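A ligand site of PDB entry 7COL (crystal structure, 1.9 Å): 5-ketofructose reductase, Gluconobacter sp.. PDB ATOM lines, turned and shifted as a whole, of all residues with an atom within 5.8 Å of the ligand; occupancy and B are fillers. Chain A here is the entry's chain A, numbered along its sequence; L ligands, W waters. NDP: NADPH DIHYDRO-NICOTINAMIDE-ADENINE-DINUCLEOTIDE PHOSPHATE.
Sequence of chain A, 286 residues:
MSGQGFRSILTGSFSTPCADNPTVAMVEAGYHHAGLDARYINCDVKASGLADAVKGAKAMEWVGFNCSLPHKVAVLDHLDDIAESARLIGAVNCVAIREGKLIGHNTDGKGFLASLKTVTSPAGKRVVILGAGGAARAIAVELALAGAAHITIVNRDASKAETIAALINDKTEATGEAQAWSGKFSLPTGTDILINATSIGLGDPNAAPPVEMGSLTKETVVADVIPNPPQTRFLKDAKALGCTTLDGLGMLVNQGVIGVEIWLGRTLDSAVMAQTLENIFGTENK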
ATOM      1  N   LYS A  72      33.241   1.974  24.145  1.00  0.00           N
ATOM      2  CA  LYS A  72      33.114   2.143  25.602  1.00  0.00           C
ATOM      3  C   LYS A  72      33.702   0.980  26.418  1.00  0.00           C
ATOM      4  O   LYS A  72      34.291   1.199  27.476  1.00  0.00           O
ATOM      5  CB  LYS A  72      31.661   2.403  25.998  1.00  0.00           C
ATOM      6  CG  LYS A  72      31.211   3.814  25.679  1.00  0.00           C
ATOM      7  CD  LYS A  72      29.774   4.063  26.087  1.00  0.00           C
ATOM      8  CE  LYS A  72      29.358   5.447  25.624  1.00  0.00           C
ATOM      9  NZ  LYS A  72      28.114   5.904  26.278  1.00  0.00           N
ATOM     10  N   ASP A 108      28.292   8.715  32.107  1.00  0.00           N
ATOM     11  CA  ASP A 108      26.930   8.424  31.646  1.00  0.00           C
ATOM     12  C   ASP A 108      25.831   8.601  32.675  1.00  0.00           C
ATOM     13  O   ASP A 108      24.735   9.071  32.341  1.00  0.00           O
ATOM     14  CB  ASP A 108      26.817   7.035  31.005  1.00  0.00           C
ATOM     15  CG  ASP A 108      27.180   7.042  29.539  1.00  0.00           C
ATOM     16  OD1 ASP A 108      26.866   8.044  28.839  1.00  0.00           O
ATOM     17  OD2 ASP A 108      27.747   6.038  29.076  1.00  0.00           O
ATOM     18  N   GLY A 111      26.056  12.918  34.749  1.00  0.00           N
ATOM     19  CA  GLY A 111      25.210  14.026  34.264  1.00  0.00           C
ATOM     20  C   GLY A 111      23.885  14.016  35.023  1.00  0.00           C
ATOM     21  O   GLY A 111      23.515  15.022  35.636  1.00  0.00           O
ATOM     22  N   PHE A 112      23.219  12.863  35.032  1.00  0.00           N
ATOM     23  CA  PHE A 112      22.024  12.664  35.842  1.00  0.00           C
ATOM     24  C   PHE A 112      22.207  13.102  37.290  1.00  0.00           C
ATOM     25  O   PHE A 112      21.383  13.859  37.798  1.00  0.00           O
ATOM     26  CB  PHE A 112      21.572  11.207  35.850  1.00  0.00           C
ATOM     27  CG  PHE A 112      20.609  10.886  36.964  1.00  0.00           C
ATOM     28  CD1 PHE A 112      19.274  11.274  36.878  1.00  0.00           C
ATOM     29  CD2 PHE A 112      21.051  10.209  38.111  1.00  0.00           C
ATOM     30  CE1 PHE A 112      18.392  10.988  37.918  1.00  0.00           C
ATOM     31  CE2 PHE A 112      20.163   9.924  39.143  1.00  0.00           C
ATOM     32  CZ  PHE A 112      18.838  10.309  39.048  1.00  0.00           C
ATOM     33  N   GLY A 131      14.061   0.684  32.866  1.00  0.00           N
ATOM     34  CA  GLY A 131      15.004   0.229  31.865  1.00  0.00           C
ATOM     35  C   GLY A 131      16.163  -0.478  32.528  1.00  0.00           C
ATOM     36  O   GLY A 131      16.410  -0.292  33.728  1.00  0.00           O
ATOM     37  N   ALA A 132      16.869  -1.299  31.751  1.00  0.00           N
ATOM     38  CA  ALA A 132      18.023  -2.059  32.209  1.00  0.00           C
ATOM     39  C   ALA A 132      19.124  -2.138  31.148  1.00  0.00           C
ATOM     40  O   ALA A 132      19.843  -3.135  31.040  1.00  0.00           O
ATOM     41  CB  ALA A 132      17.606  -3.446  32.682  1.00  0.00           C
ATOM     42  N   GLY A 133      19.265  -1.085  30.359  1.00  0.00           N
ATOM     43  CA  GLY A 133      20.348  -0.986  29.388  1.00  0.00           C
ATOM     44  C   GLY A 133      21.543  -0.287  29.987  1.00  0.00           C
ATOM     45  O   GLY A 133      21.650  -0.128  31.207  1.00  0.00           O
ATOM     46  N   GLY A 134      22.432   0.157  29.107  1.00  0.00           N
ATOM     47  CA  GLY A 134      23.633   0.881  29.498  1.00  0.00           C
ATOM     48  C   GLY A 134      23.395   2.119  30.343  1.00  0.00           C
ATOM     49  O   GLY A 134      24.144   2.375  31.276  1.00  0.00           O
ATOM     50  N   ALA A 135      22.368   2.916  30.016  1.00  0.00           N
ATOM     51  CA  ALA A 135      22.075   4.126  30.813  1.00  0.00           C
ATOM     52  C   ALA A 135      21.552   3.798  32.217  1.00  0.00           C
ATOM     53  O   ALA A 135      21.931   4.451  33.180  1.00  0.00           O
ATOM     54  CB  ALA A 135      21.075   5.019  30.088  1.00  0.00           C
ATOM     55  N   ALA A 136      20.666   2.814  32.311  1.00  0.00           N
ATOM     56  CA  ALA A 136      20.149   2.396  33.601  1.00  0.00           C
ATOM     57  C   ALA A 136      21.263   1.842  34.491  1.00  0.00           C
ATOM     58  O   ALA A 136      21.302   2.135  35.685  1.00  0.00           O
ATOM     59  CB  ALA A 136      19.048   1.366  33.415  1.00  0.00           C
ATOM     60  N   ASN A 155      12.209  -3.511  34.235  1.00  0.00           N
ATOM     61  CA  ASN A 155      12.482  -3.842  32.840  1.00  0.00           C
ATOM     62  C   ASN A 155      11.521  -4.874  32.299  1.00  0.00           C
ATOM     63  O   ASN A 155      11.048  -5.749  33.033  1.00  0.00           O
ATOM     64  CB  ASN A 155      13.918  -4.325  32.659  1.00  0.00           C
ATOM     65  CG  ASN A 155      14.447  -4.085  31.270  1.00  0.00           C
ATOM     66  OD1 ASN A 155      14.442  -2.961  30.782  1.00  0.00           O
ATOM     67  ND2 ASN A 155      14.932  -5.153  30.626  1.00  0.00           N
ATOM     68  N   ARG A 156      11.215  -4.723  31.005  1.00  0.00           N
ATOM     69  CA  ARG A 156      10.402  -5.674  30.250  1.00  0.00           C
ATOM     70  C   ARG A 156      11.047  -7.062  30.299  1.00  0.00           C
ATOM     71  O   ARG A 156      10.378  -8.045  30.669  1.00  0.00           O
ATOM     72  CB  ARG A 156      10.225  -5.149  28.816  1.00  0.00           C
ATOM     73  CG  ARG A 156       9.644  -6.100  27.775  1.00  0.00           C
ATOM     74  CD  ARG A 156      10.356  -5.877  26.456  1.00  0.00           C
ATOM     75  NE  ARG A 156       9.847  -4.722  25.717  1.00  0.00           N
ATOM     76  CZ  ARG A 156      10.596  -3.865  25.018  1.00  0.00           C
ATOM     77  NH1 ARG A 156      11.914  -3.982  24.934  1.00  0.00           N
ATOM     78  NH2 ARG A 156      10.008  -2.866  24.383  1.00  0.00           N
ATOM     79  N   ASP A 157      12.332  -7.130  29.962  1.00  0.00           N
ATOM     80  CA  ASP A 157      13.161  -8.332  30.161  1.00  0.00           C
ATOM     81  C   ASP A 157      13.699  -8.337  31.588  1.00  0.00           C
ATOM     82  O   ASP A 157      14.743  -7.744  31.864  1.00  0.00           O
ATOM     83  CB  ASP A 157      14.288  -8.371  29.119  1.00  0.00           C
ATOM     84  CG  ASP A 157      15.206  -9.605  29.244  1.00  0.00           C
ATOM     85  OD1 ASP A 157      14.973 -10.514  30.066  1.00  0.00           O
ATOM     86  OD2 ASP A 157      16.197  -9.665  28.476  1.00  0.00           O
ATOM     87  N   LYS A 160      17.424  -8.924  32.574  1.00  0.00           N
ATOM     88  CA  LYS A 160      18.318  -7.761  32.384  1.00  0.00           C
ATOM     89  C   LYS A 160      18.308  -6.867  33.624  1.00  0.00           C
ATOM     90  O   LYS A 160      19.340  -6.327  34.007  1.00  0.00           O
ATOM     91  CB  LYS A 160      17.918  -6.947  31.162  1.00  0.00           C
ATOM     92  CG  LYS A 160      18.476  -7.495  29.858  1.00  0.00           C
ATOM     93  CD  LYS A 160      18.097  -6.623  28.688  1.00  0.00           C
ATOM     94  CE  LYS A 160      19.064  -5.453  28.504  1.00  0.00           C
ATOM     95  NZ  LYS A 160      18.508  -4.444  27.562  1.00  0.00           N
ATOM     96  N   TRP A 181       8.104  -5.565  34.213  1.00  0.00           N
ATOM     97  CA  TRP A 181       7.259  -4.437  33.792  1.00  0.00           C
ATOM     98  C   TRP A 181       5.872  -4.899  33.313  1.00  0.00           C
ATOM     99  O   TRP A 181       5.576  -4.894  32.115  1.00  0.00           O
ATOM    100  CB  TRP A 181       7.965  -3.575  32.718  1.00  0.00           C
ATOM    101  CG  TRP A 181       7.455  -2.151  32.653  1.00  0.00           C
ATOM    102  CD1 TRP A 181       6.236  -1.678  33.057  1.00  0.00           C
ATOM    103  CD2 TRP A 181       8.158  -1.023  32.126  1.00  0.00           C
ATOM    104  NE1 TRP A 181       6.138  -0.331  32.825  1.00  0.00           N
ATOM    105  CE2 TRP A 181       7.302   0.105  32.251  1.00  0.00           C
ATOM    106  CE3 TRP A 181       9.429  -0.840  31.563  1.00  0.00           C
ATOM    107  CZ2 TRP A 181       7.683   1.388  31.838  1.00  0.00           C
ATOM    108  CZ3 TRP A 181       9.815   0.436  31.146  1.00  0.00           C
ATOM    109  CH2 TRP A 181       8.932   1.542  31.291  1.00  0.00           C
ATOM    110  N   ALA A 197      15.033   5.572  32.059  1.00  0.00           N
ATOM    111  CA  ALA A 197      16.309   5.245  31.390  1.00  0.00           C
ATOM    112  C   ALA A 197      16.131   4.314  30.195  1.00  0.00           C
ATOM    113  O   ALA A 197      17.097   3.794  29.656  1.00  0.00           O
ATOM    114  CB  ALA A 197      17.310   4.680  32.394  1.00  0.00           C
ATOM    115  N   THR A 198      14.879   4.147  29.758  1.00  0.00           N
ATOM    116  CA  THR A 198      14.557   3.512  28.469  1.00  0.00           C
ATOM    117  C   THR A 198      14.788   4.524  27.336  1.00  0.00           C
ATOM    118  O   THR A 198      15.021   5.715  27.584  1.00  0.00           O
ATOM    119  CB  THR A 198      13.078   3.046  28.383  1.00  0.00           C
ATOM    120  OG1 THR A 198      12.204   4.180  28.369  1.00  0.00           O
ATOM    121  CG2 THR A 198      12.694   2.118  29.541  1.00  0.00           C
ATOM    122  N   SER A 199      14.697   4.049  26.093  1.00  0.00           N
ATOM    123  CA  SER A 199      14.753   4.894  24.882  1.00  0.00           C
ATOM    124  C   SER A 199      13.368   5.420  24.436  1.00  0.00           C
ATOM    125  O   SER A 199      13.255   6.113  23.412  1.00  0.00           O
ATOM    126  CB  SER A 199      15.449   4.145  23.747  1.00  0.00           C
ATOM    127  OG  SER A 199      14.842   2.875  23.547  1.00  0.00           O
ATOM    128  N   ILE A 200      12.313   5.064  25.186  1.00  0.00           N
ATOM    129  CA  ILE A 200      10.958   5.555  24.905  1.00  0.00           C
ATOM    130  C   ILE A 200      10.975   7.092  24.954  1.00  0.00           C
ATOM    131  O   ILE A 200      11.440   7.670  25.933  1.00  0.00           O
ATOM    132  CB  ILE A 200       9.915   5.011  25.926  1.00  0.00           C
ATOM    133  CG1 ILE A 200       9.878   3.476  25.931  1.00  0.00           C
ATOM    134  CG2 ILE A 200       8.520   5.589  25.645  1.00  0.00           C
ATOM    135  CD1 ILE A 200       8.874   2.854  26.902  1.00  0.00           C
ATOM    136  N   LEU A 202      12.550   9.051  22.642  1.00  0.00           N
ATOM    137  CA  LEU A 202      13.699   9.581  21.869  1.00  0.00           C
ATOM    138  C   LEU A 202      13.256  10.086  20.492  1.00  0.00           C
ATOM    139  O   LEU A 202      12.853   9.289  19.640  1.00  0.00           O
ATOM    140  CB  LEU A 202      14.835   8.542  21.759  1.00  0.00           C
ATOM    141  CG  LEU A 202      16.175   8.983  21.147  1.00  0.00           C
ATOM    142  CD1 LEU A 202      16.859  10.094  21.940  1.00  0.00           C
ATOM    143  CD2 LEU A 202      17.111   7.794  21.004  1.00  0.00           C
ATOM    144  N   PRO A 210       4.983   3.065  29.977  1.00  0.00           N
ATOM    145  CA  PRO A 210       3.728   2.607  30.584  1.00  0.00           C
ATOM    146  C   PRO A 210       3.763   2.648  32.121  1.00  0.00           C
ATOM    147  O   PRO A 210       4.134   1.676  32.791  1.00  0.00           O
ATOM    148  CB  PRO A 210       3.534   1.178  30.030  1.00  0.00           C
ATOM    149  CG  PRO A 210       4.855   0.784  29.448  1.00  0.00           C
ATOM    150  CD  PRO A 210       5.563   2.040  29.067  1.00  0.00           C
ATOM    151  N   ASP A 224      14.361  12.092  33.386  1.00  0.00           N
ATOM    152  CA  ASP A 224      14.303  11.420  32.114  1.00  0.00           C
ATOM    153  C   ASP A 224      15.632  11.612  31.378  1.00  0.00           C
ATOM    154  O   ASP A 224      16.119  12.733  31.252  1.00  0.00           O
ATOM    155  CB  ASP A 224      13.143  11.996  31.288  1.00  0.00           C
ATOM    156  CG  ASP A 224      12.705  11.068  30.185  1.00  0.00           C
ATOM    157  OD1 ASP A 224      13.572  10.403  29.574  1.00  0.00           O
ATOM    158  OD2 ASP A 224      11.488  10.997  29.919  1.00  0.00           O
ATOM    159  N   VAL A 225      16.176  10.508  30.875  1.00  0.00           N
ATOM    160  CA  VAL A 225      17.471  10.524  30.203  1.00  0.00           C
ATOM    161  C   VAL A 225      17.424  11.144  28.827  1.00  0.00           C
ATOM    162  O   VAL A 225      18.461  11.628  28.332  1.00  0.00           O
ATOM    163  CB  VAL A 225      18.153   9.129  30.172  1.00  0.00           C
ATOM    164  CG1 VAL A 225      18.461   8.677  31.583  1.00  0.00           C
ATOM    165  CG2 VAL A 225      17.315   8.084  29.443  1.00  0.00           C
ATOM    166  N   ILE A 226      16.237  11.143  28.197  1.00  0.00           N
ATOM    167  CA  ILE A 226      16.080  11.580  26.793  1.00  0.00           C
ATOM    168  C   ILE A 226      16.531  13.033  26.580  1.00  0.00           C
ATOM    169  O   ILE A 226      15.962  13.941  27.177  1.00  0.00           O
ATOM    170  CB  ILE A 226      14.674  11.256  26.199  1.00  0.00           C
ATOM    171  CG1 ILE A 226      14.676   9.848  25.593  1.00  0.00           C
ATOM    172  CG2 ILE A 226      14.312  12.183  25.031  1.00  0.00           C
ATOM    173  CD1 ILE A 226      14.356   8.738  26.559  1.00  0.00           C
ATOM    174  N   PRO A 227      17.576  13.224  25.737  1.00  0.00           N
ATOM    175  CA  PRO A 227      18.084  14.580  25.535  1.00  0.00           C
ATOM    176  C   PRO A 227      17.206  15.406  24.580  1.00  0.00           C
ATOM    177  O   PRO A 227      17.122  16.633  24.738  1.00  0.00           O
ATOM    178  CB  PRO A 227      19.490  14.365  24.963  1.00  0.00           C
ATOM    179  CG  PRO A 227      19.496  12.988  24.395  1.00  0.00           C
ATOM    180  CD  PRO A 227      18.361  12.202  25.010  1.00  0.00           C
ATOM    181  N   GLY A 248      16.791  15.267  30.086  1.00  0.00           N
ATOM    182  CA  GLY A 248      18.009  14.636  29.607  1.00  0.00           C
ATOM    183  C   GLY A 248      18.947  15.613  28.894  1.00  0.00           C
ATOM    184  O   GLY A 248      20.135  15.315  28.758  1.00  0.00           O
ATOM    185  N   LEU A 249      18.432  16.767  28.468  1.00  0.00           N
ATOM    186  CA  LEU A 249      19.289  17.829  27.878  1.00  0.00           C
ATOM    187  C   LEU A 249      20.213  18.408  28.939  1.00  0.00           C
ATOM    188  O   LEU A 249      21.422  18.546  28.704  1.00  0.00           O
ATOM    189  CB  LEU A 249      18.445  18.947  27.186  1.00  0.00           C
ATOM    190  CG  LEU A 249      19.117  20.045  26.323  1.00  0.00           C
ATOM    191  CD1 LEU A 249      18.158  20.568  25.269  1.00  0.00           C
ATOM    192  CD2 LEU A 249      19.638  21.209  27.172  1.00  0.00           C
ATOM    193  N   MET A 251      21.146  16.904  31.619  1.00  0.00           N
ATOM    194  CA  MET A 251      22.057  15.782  31.936  1.00  0.00           C
ATOM    195  C   MET A 251      23.253  15.702  31.004  1.00  0.00           C
ATOM    196  O   MET A 251      24.374  15.439  31.436  1.00  0.00           O
ATOM    197  CB  MET A 251      21.279  14.463  31.933  1.00  0.00           C
ATOM    198  CG  MET A 251      20.249  14.410  33.044  1.00  0.00           C
ATOM    199  SD  MET A 251      19.360  12.855  32.996  1.00  0.00           S
ATOM    200  CE  MET A 251      17.933  13.221  34.006  1.00  0.00           C
ATOM    201  N   LEU A 252      23.010  15.928  29.716  1.00  0.00           N
ATOM    202  CA  LEU A 252      24.079  15.940  28.712  1.00  0.00           C
ATOM    203  C   LEU A 252      25.034  17.118  28.922  1.00  0.00           C
ATOM    204  O   LEU A 252      26.248  16.956  28.828  1.00  0.00           O
ATOM    205  CB  LEU A 252      23.511  15.996  27.299  1.00  0.00           C
ATOM    206  CG  LEU A 252      24.091  15.113  26.183  1.00  0.00           C
ATOM    207  CD1 LEU A 252      23.526  15.589  24.850  1.00  0.00           C
ATOM    208  CD2 LEU A 252      25.617  15.079  26.130  1.00  0.00           C
ATOM    209  N   GLN A 255      27.243  16.160  31.882  1.00  0.00           N
ATOM    210  CA  GLN A 255      28.273  15.255  31.391  1.00  0.00           C
ATOM    211  C   GLN A 255      29.438  15.996  30.749  1.00  0.00           C
ATOM    212  O   GLN A 255      30.593  15.642  30.969  1.00  0.00           O
ATOM    213  CB  GLN A 255      27.709  14.312  30.323  1.00  0.00           C
ATOM    214  CG  GLN A 255      26.927  13.119  30.832  1.00  0.00           C
ATOM    215  CD  GLN A 255      27.029  11.941  29.869  1.00  0.00           C
ATOM    216  OE1 GLN A 255      28.103  11.398  29.653  1.00  0.00           O
ATOM    217  NE2 GLN A 255      25.897  11.530  29.331  1.00  0.00           N
HETATM  218  PA  NDP L   1      19.944   0.450  25.527  1.00  0.00           P
HETATM  219  O1A NDP L   1      19.574  -0.017  24.135  1.00  0.00           O
HETATM  220  O2A NDP L   1      21.220  -0.058  26.164  1.00  0.00           O
HETATM  221  O5B NDP L   1      18.723   0.107  26.526  1.00  0.00           O
HETATM  222  C5B NDP L   1      17.376   0.406  26.147  1.00  0.00           C
HETATM  223  C4B NDP L   1      16.457   0.162  27.322  1.00  0.00           C
HETATM  224  O4B NDP L   1      15.179   0.732  27.051  1.00  0.00           O
HETATM  225  C3B NDP L   1      16.208  -1.316  27.564  1.00  0.00           C
HETATM  226  O3B NDP L   1      16.130  -1.559  28.979  1.00  0.00           O
HETATM  227  C2B NDP L   1      14.851  -1.572  26.948  1.00  0.00           C
HETATM  228  O2B NDP L   1      14.158  -2.691  27.519  1.00  0.00           O
HETATM  229  C1B NDP L   1      14.142  -0.253  27.201  1.00  0.00           C
HETATM  230  N9A NDP L   1      13.039  -0.018  26.240  1.00  0.00           N
HETATM  231  C8A NDP L   1      13.176   0.488  24.990  1.00  0.00           C
HETATM  232  N7A NDP L   1      11.972   0.570  24.368  1.00  0.00           N
HETATM  233  C5A NDP L   1      11.046   0.120  25.250  1.00  0.00           C
HETATM  234  C6A NDP L   1       9.573  -0.064  25.258  1.00  0.00           C
HETATM  235  N6A NDP L   1       8.849   0.269  24.156  1.00  0.00           N
HETATM  236  N1A NDP L   1       8.980  -0.569  26.371  1.00  0.00           N
HETATM  237  C2A NDP L   1       9.684  -0.906  27.462  1.00  0.00           C
HETATM  238  N3A NDP L   1      11.024  -0.760  27.533  1.00  0.00           N
HETATM  239  C4A NDP L   1      11.755  -0.264  26.476  1.00  0.00           C
HETATM  240  O3  NDP L   1      19.922   2.065  25.549  1.00  0.00           O
HETATM  241  PN  NDP L   1      20.801   2.941  26.592  1.00  0.00           P
HETATM  242  O1N NDP L   1      22.222   3.010  26.067  1.00  0.00           O
HETATM  243  O2N NDP L   1      20.539   2.421  27.978  1.00  0.00           O
HETATM  244  O5D NDP L   1      20.185   4.433  26.476  1.00  0.00           O
HETATM  245  C5D NDP L   1      18.798   4.721  26.693  1.00  0.00           C
HETATM  246  C4D NDP L   1      18.512   6.183  26.350  1.00  0.00           C
HETATM  247  O4D NDP L   1      19.214   7.045  27.238  1.00  0.00           O
HETATM  248  C3D NDP L   1      18.960   6.553  24.933  1.00  0.00           C
HETATM  249  O3D NDP L   1      17.829   7.139  24.276  1.00  0.00           O
HETATM  250  C2D NDP L   1      20.110   7.543  25.103  1.00  0.00           C
HETATM  251  O2D NDP L   1      20.017   8.600  24.141  1.00  0.00           O
HETATM  252  C1D NDP L   1      19.920   8.069  26.522  1.00  0.00           C
HETATM  253  N1N NDP L   1      21.136   8.488  27.263  1.00  0.00           N
HETATM  254  C2N NDP L   1      21.161   9.756  27.734  1.00  0.00           C
HETATM  255  C3N NDP L   1      22.253  10.264  28.464  1.00  0.00           C
HETATM  256  C7N NDP L   1      22.239  11.708  28.953  1.00  0.00           C
HETATM  257  O7N NDP L   1      23.233  12.191  29.504  1.00  0.00           O
HETATM  258  N7N NDP L   1      21.132  12.447  28.776  1.00  0.00           N
HETATM  259  C4N NDP L   1      23.331   9.392  28.719  1.00  0.00           C
HETATM  260  C5N NDP L   1      23.284   8.078  28.249  1.00  0.00           C
HETATM  261  C6N NDP L   1      22.166   7.641  27.519  1.00  0.00           C
HETATM  262  P2B NDP L   1      14.572  -4.200  27.142  1.00  0.00           P
HETATM  263  O1X NDP L   1      15.780  -4.448  28.031  1.00  0.00           O
HETATM  264  O2X NDP L   1      13.359  -5.018  27.534  1.00  0.00           O
HETATM  265  O3X NDP L   1      14.871  -4.159  25.665  1.00  0.00           O
HETATM  266  O   HOH W   1       9.984   0.662  21.629  1.00  0.00           O
HETATM  267  O   HOH W   2      24.215  11.507  32.641  1.00  0.00           O
HETATM  268  O   HOH W   3      20.457  -3.271  26.328  1.00  0.00           O
HETATM  269  O   HOH W   4       6.417  -1.308  22.569  1.00  0.00           O
HETATM  270  O   HOH W   5      24.528   1.221  26.147  1.00  0.00           O
HETATM  271  O   HOH W   6      18.935   1.663  30.032  1.00  0.00           O
HETATM  272  O   HOH W   7       6.871  -2.000  28.994  1.00  0.00           O
HETATM  273  O   HOH W   8      11.891   2.438  22.036  1.00  0.00           O
HETATM  274  O   HOH W   9      11.881  -2.070  30.019  1.00  0.00           O
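An oxygen (O1X) of the ligand is in salt-bridge range of the side-chain amino group (NZ) of Lys 160 (2.8 Å). The backbone NH (N) of Gly 133 sits at hydrogen-bond distance from an oxygen (O3B) of the ligand (3.5 Å). An oxygen (O2X) of the ligand is in hydrogen-bond range of the backbone NH of Asp 157, at 3.4 Å. NE2 of Gln 255 sits at hydrogen-bond distance from O7N of the ligand, 2.8 Å away. O of Val 225 sits at hydrogen-bond distance from N7N of the ligand (2.8 Å). N of Ser 199 sits at hydrogen-bond distance from O4B of the ligand. The backbone NH of Gly 134 is in hydrogen-bond range of an oxygen (O2N) of the ligand. O2N of the ligand lies within hydrogen-bond range of N of Ala 135, at 2.8 Å. N of Ala 132 sits at hydrogen-bond distance from O3B of the ligand (2.9 Å). O1X of the ligand sits at hydrogen-bond distance from ND2 of Asn 155 (2.8 Å). The guanidinium group of Arg 156 lies within salt-bridge range of an oxygen (O3X) of the ligand, at 3.1 Å. N7N of the ligand lies within hydrogen-bond range of O of Gly 248 (3.0 Å).
Water W6 lies within hydrogen-bond range of an oxygen (O2N) of the ligand (2.7 Å), the backbone NH (N) of Gly 133 (2.8 Å), the backbone carbonyl oxygen (O) of Ala 197 (2.8 Å) and the backbone NH (N) of Ala 136 (3.1 Å). Water W9 lies within hydrogen-bond range of the side-chain amide oxygen of Asn 155 (2.8 Å), the backbone NH of Arg 156 (2.9 Å) and a nitrogen (N3A) of the ligand (2.9 Å). Water W8 bridges a nitrogen (N7A) of the ligand (3.0 Å) and the side-chain hydroxyl (OG) of Ser 199 (3.3 Å). Water W3 bridges NZ of Lys 160 and O2A of the ligand. Water W2 lies within hydrogen-bond range of the backbone carbonyl oxygen (O) of Asp 108 (2.5 Å), the backbone NH (N) of Phe 112 (2.9 Å), the backbone NH (N) of Gly 111 (3.1 Å) and an oxygen (O7N) of the ligand (3.4 Å).
Residues that only touch the ligand: Asp 108 (3.6 Å), Gly 131 (3.6 Å), Trp 181 (3.9 Å), Ala 197 (3.5 Å), Thr 198 (3.2 Å), Ile 200 (3.4 Å), Leu 202 (3.4 Å), Met 251 (3.7 Å) and Leu 252 (3.7 Å). Hydrophobic or aromatic side chains within 4 Å of the ligand: Ala 135, Trp 181, Ile 200, Leu 202, Val 225 and Met 251. Of the 30 residues printed, 21 come within 4 Å of the ligand. The nearest printed residue that does not touch the ligand is Pro 227 (4.1 Å).
NZ of Lys 72 lies within salt-bridge range of OD2 of Asp 108, at 2.8 Å. The backbone NH of Gly 248 lies close to the backbone carbonyl oxygen of Ile 226 (3.3 Å). The backbone NH of Gly 248 is in hydrogen-bond range of the backbone carbonyl oxygen of Asp 224 (2.9 Å). The side-chain amide oxygen of Asn 155 is in hydrogen-bond range of the backbone NH of Ala 132 (3.1 Å). The side-chain hydroxyl (OG1) of Thr 198 sits at hydrogen-bond distance from the backbone NH (N) of Ile 200. The backbone carbonyl oxygen (O) of Pro 210 is in hydrogen-bond range of the indole nitrogen (NE1) of Trp 181 (2.8 Å). O of Asn 155 lies within hydrogen-bond range of N of Trp 181 (3.2 Å). The backbone carbonyl oxygen (O) of Asp 157 lies within hydrogen-bond range of the side-chain amide nitrogen (ND2) of Asn 155, at 2.9 Å.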
